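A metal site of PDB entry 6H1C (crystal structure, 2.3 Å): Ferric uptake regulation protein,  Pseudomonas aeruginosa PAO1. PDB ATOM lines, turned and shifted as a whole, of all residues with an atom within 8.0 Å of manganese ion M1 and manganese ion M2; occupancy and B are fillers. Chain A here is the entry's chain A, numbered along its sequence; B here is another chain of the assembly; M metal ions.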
ATOM      1  N   SER A  34     -22.018 -26.136 -11.236  1.00  0.00           N
ATOM      2  CA  SER A  34     -21.818 -24.689 -11.119  1.00  0.00           C
ATOM      3  C   SER A  34     -22.136 -24.231  -9.701  1.00  0.00           C
ATOM      4  O   SER A  34     -22.681 -24.978  -8.883  1.00  0.00           O
ATOM      5  CB  SER A  34     -22.711 -23.940 -12.096  1.00  0.00           C
ATOM      6  OG  SER A  34     -24.050 -23.954 -11.654  1.00  0.00           O
ATOM      7  N   ASN A  71     -13.479 -23.788 -16.558  1.00  0.00           N
ATOM      8  CA  ASN A  71     -14.443 -23.024 -17.356  1.00  0.00           C
ATOM      9  C   ASN A  71     -14.479 -23.683 -18.733  1.00  0.00           C
ATOM     10  O   ASN A  71     -13.680 -23.346 -19.601  1.00  0.00           O
ATOM     11  CB  ASN A  71     -14.056 -21.563 -17.438  1.00  0.00           C
ATOM     12  CG  ASN A  71     -15.156 -20.712 -18.051  1.00  0.00           C
ATOM     13  OD1 ASN A  71     -15.603 -20.988 -19.154  1.00  0.00           O
ATOM     14  ND2 ASN A  71     -15.622 -19.717 -17.317  1.00  0.00           N
ATOM     15  N   PHE A  72     -15.399 -24.621 -18.928  1.00  0.00           N
ATOM     16  CA  PHE A  72     -15.328 -25.450 -20.123  1.00  0.00           C
ATOM     17  C   PHE A  72     -15.944 -24.752 -21.320  1.00  0.00           C
ATOM     18  O   PHE A  72     -15.355 -24.723 -22.407  1.00  0.00           O
ATOM     19  CB  PHE A  72     -15.998 -26.808 -19.914  1.00  0.00           C
ATOM     20  CG  PHE A  72     -15.249 -27.705 -18.959  1.00  0.00           C
ATOM     21  CD1 PHE A  72     -13.966 -28.102 -19.238  1.00  0.00           C
ATOM     22  CD2 PHE A  72     -15.843 -28.160 -17.819  1.00  0.00           C
ATOM     23  CE1 PHE A  72     -13.284 -28.927 -18.387  1.00  0.00           C
ATOM     24  CE2 PHE A  72     -15.166 -28.980 -16.961  1.00  0.00           C
ATOM     25  CZ  PHE A  72     -13.885 -29.362 -17.252  1.00  0.00           C
ATOM     26  N   ASP A  73     -17.123 -24.152 -21.151  1.00  0.00           N
ATOM     27  CA  ASP A  73     -17.778 -23.553 -22.301  1.00  0.00           C
ATOM     28  C   ASP A  73     -17.572 -22.055 -22.395  1.00  0.00           C
ATOM     29  O   ASP A  73     -18.219 -21.411 -23.219  1.00  0.00           O
ATOM     30  CB  ASP A  73     -19.266 -23.890 -22.304  1.00  0.00           C
ATOM     31  CG  ASP A  73     -20.025 -23.246 -21.183  1.00  0.00           C
ATOM     32  OD1 ASP A  73     -19.526 -22.267 -20.572  1.00  0.00           O
ATOM     33  OD2 ASP A  73     -21.146 -23.730 -20.920  1.00  0.00           O
ATOM     34  N   GLY A  74     -16.666 -21.478 -21.600  1.00  0.00           N
ATOM     35  CA  GLY A  74     -16.405 -20.055 -21.621  1.00  0.00           C
ATOM     36  C   GLY A  74     -17.302 -19.211 -20.736  1.00  0.00           C
ATOM     37  O   GLY A  74     -16.914 -18.108 -20.347  1.00  0.00           O
ATOM     38  N   GLY A  75     -18.486 -19.714 -20.387  1.00  0.00           N
ATOM     39  CA  GLY A  75     -19.491 -18.889 -19.757  1.00  0.00           C
ATOM     40  C   GLY A  75     -19.635 -19.035 -18.256  1.00  0.00           C
ATOM     41  O   GLY A  75     -19.859 -18.043 -17.580  1.00  0.00           O
ATOM     42  N   HIS A  76     -19.522 -20.242 -17.717  1.00  0.00           N
ATOM     43  CA  HIS A  76     -19.757 -20.460 -16.301  1.00  0.00           C
ATOM     44  C   HIS A  76     -18.656 -21.333 -15.699  1.00  0.00           C
ATOM     45  O   HIS A  76     -18.007 -22.126 -16.386  1.00  0.00           O
ATOM     46  CB  HIS A  76     -21.122 -21.084 -16.043  1.00  0.00           C
ATOM     47  CG  HIS A  76     -21.141 -22.567 -16.149  1.00  0.00           C
ATOM     48  ND1 HIS A  76     -21.251 -23.227 -17.352  1.00  0.00           N
ATOM     49  CD2 HIS A  76     -21.104 -23.532 -15.200  1.00  0.00           C
ATOM     50  CE1 HIS A  76     -21.258 -24.530 -17.143  1.00  0.00           C
ATOM     51  NE2 HIS A  76     -21.170 -24.742 -15.840  1.00  0.00           N
ATOM     52  N   ALA A  77     -18.452 -21.151 -14.401  1.00  0.00           N
ATOM     53  CA  ALA A  77     -17.406 -21.850 -13.669  1.00  0.00           C
ATOM     54  C   ALA A  77     -17.915 -23.198 -13.181  1.00  0.00           C
ATOM     55  O   ALA A  77     -19.039 -23.308 -12.681  1.00  0.00           O
ATOM     56  CB  ALA A  77     -16.914 -21.017 -12.484  1.00  0.00           C
ATOM     57  N   VAL A  78     -17.073 -24.217 -13.323  1.00  0.00           N
ATOM     58  CA  VAL A  78     -17.363 -25.581 -12.871  1.00  0.00           C
ATOM     59  C   VAL A  78     -16.480 -25.895 -11.678  1.00  0.00           C
ATOM     60  O   VAL A  78     -15.259 -25.695 -11.721  1.00  0.00           O
ATOM     61  CB  VAL A  78     -17.083 -26.610 -13.991  1.00  0.00           C
ATOM     62  CG1 VAL A  78     -16.827 -27.993 -13.379  1.00  0.00           C
ATOM     63  CG2 VAL A  78     -18.240 -26.646 -14.976  1.00  0.00           C
ATOM     64  N   THR A  95     -22.242 -28.800 -28.009  1.00  0.00           N
ATOM     65  CA  THR A  95     -23.233 -28.944 -26.957  1.00  0.00           C
ATOM     66  C   THR A  95     -22.733 -28.568 -25.567  1.00  0.00           C
ATOM     67  O   THR A  95     -23.545 -28.291 -24.693  1.00  0.00           O
ATOM     68  CB  THR A  95     -23.744 -30.380 -26.912  1.00  0.00           C
ATOM     69  OG1 THR A  95     -22.657 -31.271 -26.617  1.00  0.00           O
ATOM     70  CG2 THR A  95     -24.378 -30.766 -28.252  1.00  0.00           C
ATOM     71  N   GLY A  96     -21.418 -28.537 -25.341  1.00  0.00           N
ATOM     72  CA  GLY A  96     -20.909 -28.417 -23.996  1.00  0.00           C
ATOM     73  C   GLY A  96     -20.939 -29.702 -23.201  1.00  0.00           C
ATOM     74  O   GLY A  96     -20.741 -29.664 -21.982  1.00  0.00           O
ATOM     75  N   SER B  34     -27.225 -15.916 -19.771  1.00  0.00           N
ATOM     76  CA  SER B  34     -25.976 -16.643 -19.919  1.00  0.00           C
ATOM     77  C   SER B  34     -25.740 -17.042 -21.374  1.00  0.00           C
ATOM     78  O   SER B  34     -26.640 -17.015 -22.212  1.00  0.00           O
ATOM     79  CB  SER B  34     -26.008 -17.896 -19.052  1.00  0.00           C
ATOM     80  OG  SER B  34     -26.734 -18.927 -19.693  1.00  0.00           O
ATOM     81  N   ALA B  35     -24.493 -17.415 -21.678  1.00  0.00           N
ATOM     82  CA  ALA B  35     -24.234 -17.986 -22.998  1.00  0.00           C
ATOM     83  C   ALA B  35     -25.096 -19.220 -23.234  1.00  0.00           C
ATOM     84  O   ALA B  35     -25.570 -19.454 -24.343  1.00  0.00           O
ATOM     85  CB  ALA B  35     -22.754 -18.331 -23.143  1.00  0.00           C
ATOM     86  N   GLU B  36     -25.297 -20.028 -22.198  1.00  0.00           N
ATOM     87  CA  GLU B  36     -26.144 -21.211 -22.326  1.00  0.00           C
ATOM     88  C   GLU B  36     -27.589 -20.828 -22.622  1.00  0.00           C
ATOM     89  O   GLU B  36     -28.257 -21.485 -23.424  1.00  0.00           O
ATOM     90  CB  GLU B  36     -26.056 -22.064 -21.059  1.00  0.00           C
ATOM     91  CG  GLU B  36     -25.004 -23.148 -21.058  1.00  0.00           C
ATOM     92  CD  GLU B  36     -25.158 -24.096 -19.868  1.00  0.00           C
ATOM     93  OE1 GLU B  36     -26.154 -24.848 -19.802  1.00  0.00           O
ATOM     94  OE2 GLU B  36     -24.296 -24.066 -18.983  1.00  0.00           O
ATOM     95  N   ASP B  37     -28.091 -19.763 -21.985  1.00  0.00           N
ATOM     96  CA  ASP B  37     -29.436 -19.265 -22.290  1.00  0.00           C
ATOM     97  C   ASP B  37     -29.587 -18.897 -23.755  1.00  0.00           C
ATOM     98  O   ASP B  37     -30.630 -19.147 -24.359  1.00  0.00           O
ATOM     99  CB  ASP B  37     -29.757 -18.051 -21.447  1.00  0.00           C
ATOM    100  CG  ASP B  37     -29.816 -18.351 -19.978  1.00  0.00           C
ATOM    101  OD1 ASP B  37     -30.090 -19.535 -19.644  1.00  0.00           O
ATOM    102  OD2 ASP B  37     -29.606 -17.410 -19.173  1.00  0.00           O
ATOM    103  N   LYS B  40     -29.626 -22.252 -25.773  1.00  0.00           N
ATOM    104  CA  LYS B  40     -30.927 -22.900 -25.623  1.00  0.00           C
ATOM    105  C   LYS B  40     -31.988 -22.162 -26.432  1.00  0.00           C
ATOM    106  O   LYS B  40     -32.769 -22.790 -27.158  1.00  0.00           O
ATOM    107  CB  LYS B  40     -31.321 -22.969 -24.148  1.00  0.00           C
ATOM    108  CG  LYS B  40     -30.288 -23.663 -23.264  1.00  0.00           C
ATOM    109  CD  LYS B  40     -30.755 -23.850 -21.790  1.00  0.00           C
ATOM    110  CE  LYS B  40     -29.643 -24.507 -20.926  1.00  0.00           C
ATOM    111  NZ  LYS B  40     -29.967 -24.667 -19.482  1.00  0.00           N
ATOM    112  N   LEU B  51     -22.730 -24.165 -29.084  1.00  0.00           N
ATOM    113  CA  LEU B  51     -22.391 -23.410 -27.880  1.00  0.00           C
ATOM    114  C   LEU B  51     -21.076 -22.654 -28.044  1.00  0.00           C
ATOM    115  O   LEU B  51     -20.966 -21.481 -27.652  1.00  0.00           O
ATOM    116  CB  LEU B  51     -22.318 -24.379 -26.704  1.00  0.00           C
ATOM    117  CG  LEU B  51     -22.143 -23.822 -25.307  1.00  0.00           C
ATOM    118  CD1 LEU B  51     -23.155 -22.733 -25.071  1.00  0.00           C
ATOM    119  CD2 LEU B  51     -22.333 -24.948 -24.312  1.00  0.00           C
ATOM    120  N   TYR B  55     -20.727 -18.466 -27.696  1.00  0.00           N
ATOM    121  CA  TYR B  55     -19.849 -17.740 -26.791  1.00  0.00           C
ATOM    122  C   TYR B  55     -18.889 -16.843 -27.551  1.00  0.00           C
ATOM    123  O   TYR B  55     -18.637 -15.710 -27.127  1.00  0.00           O
ATOM    124  CB  TYR B  55     -19.085 -18.724 -25.916  1.00  0.00           C
ATOM    125  CG  TYR B  55     -18.105 -18.036 -25.033  1.00  0.00           C
ATOM    126  CD1 TYR B  55     -18.530 -17.336 -23.902  1.00  0.00           C
ATOM    127  CD2 TYR B  55     -16.751 -18.068 -25.310  1.00  0.00           C
ATOM    128  CE1 TYR B  55     -17.622 -16.675 -23.084  1.00  0.00           C
ATOM    129  CE2 TYR B  55     -15.853 -17.403 -24.501  1.00  0.00           C
ATOM    130  CZ  TYR B  55     -16.289 -16.713 -23.396  1.00  0.00           C
ATOM    131  OH  TYR B  55     -15.379 -16.074 -22.589  1.00  0.00           O
ATOM    132  N   GLY B  75     -20.019 -16.738 -10.614  1.00  0.00           N
ATOM    133  CA  GLY B  75     -19.902 -18.075 -11.163  1.00  0.00           C
ATOM    134  C   GLY B  75     -20.282 -18.237 -12.620  1.00  0.00           C
ATOM    135  O   GLY B  75     -19.961 -19.269 -13.224  1.00  0.00           O
ATOM    136  N   HIS B  76     -20.952 -17.242 -13.217  1.00  0.00           N
ATOM    137  CA  HIS B  76     -21.265 -17.322 -14.637  1.00  0.00           C
ATOM    138  C   HIS B  76     -21.418 -15.921 -15.201  1.00  0.00           C
ATOM    139  O   HIS B  76     -21.806 -14.981 -14.504  1.00  0.00           O
ATOM    140  CB  HIS B  76     -22.534 -18.162 -14.890  1.00  0.00           C
ATOM    141  CG  HIS B  76     -23.826 -17.415 -14.741  1.00  0.00           C
ATOM    142  ND1 HIS B  76     -24.511 -17.319 -13.542  1.00  0.00           N
ATOM    143  CD2 HIS B  76     -24.562 -16.719 -15.641  1.00  0.00           C
ATOM    144  CE1 HIS B  76     -25.597 -16.592 -13.719  1.00  0.00           C
ATOM    145  NE2 HIS B  76     -25.656 -16.217 -14.972  1.00  0.00           N
ATOM    146  N   ALA B  77     -21.131 -15.784 -16.488  1.00  0.00           N
ATOM    147  CA  ALA B  77     -21.148 -14.513 -17.179  1.00  0.00           C
ATOM    148  C   ALA B  77     -22.539 -14.194 -17.724  1.00  0.00           C
ATOM    149  O   ALA B  77     -23.229 -15.053 -18.274  1.00  0.00           O
ATOM    150  CB  ALA B  77     -20.122 -14.511 -18.300  1.00  0.00           C
HETATM  151 MN    MN M   1     -22.607 -22.734 -19.292  1.00  0.00          MN
HETATM  152 MN    MN M   2     -21.766 -22.491 -19.211  1.00  0.00          MN
HETATM  153 MN    MN M   3     -22.815 -20.312 -19.453  1.00  0.00          MN
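The backbone NH (N) of Glu 36 of chain B sits at hydrogen-bond distance from the side-chain hydroxyl (OG) of Ser 34 of chain B (3.1 Å). The side-chain carboxylate (OE1) of Glu 36 of chain B lies within salt-bridge range of the side-chain amino group (NZ) of Lys 40 of chain B (3.8 Å). The backbone NH (N) of Gly 75 of chain A lies close to the side-chain carboxylate (OD1) of Asp 73 (2.8 Å).
The nearest printed residue that does not touch manganese ion M1 is Gly 75 of chain A (4.9 Å).
Within 4 Å of manganese ion M2: Asp 73, His 76 of chain A and Glu 36 of chain B. The nearest printed residue that does not touch manganese ion M2 is Gly 75 of chain A (4.2 Å).
OE2 of Glu 36 of chain B is bound to manganese ion M1. The side-chain carboxylate (OD2) of Asp 73 binds manganese ion M1 (2.4 Å). ND1 of His 76 of chain A is bound to manganese ion M1, 2.4 Å away.
Manganese ion M2 is bound by ND1 of His 76 of chain A, OD2 of Asp 73 and OD1 of Asp 73. Manganese ion M2 has three donor atoms within binding distance.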
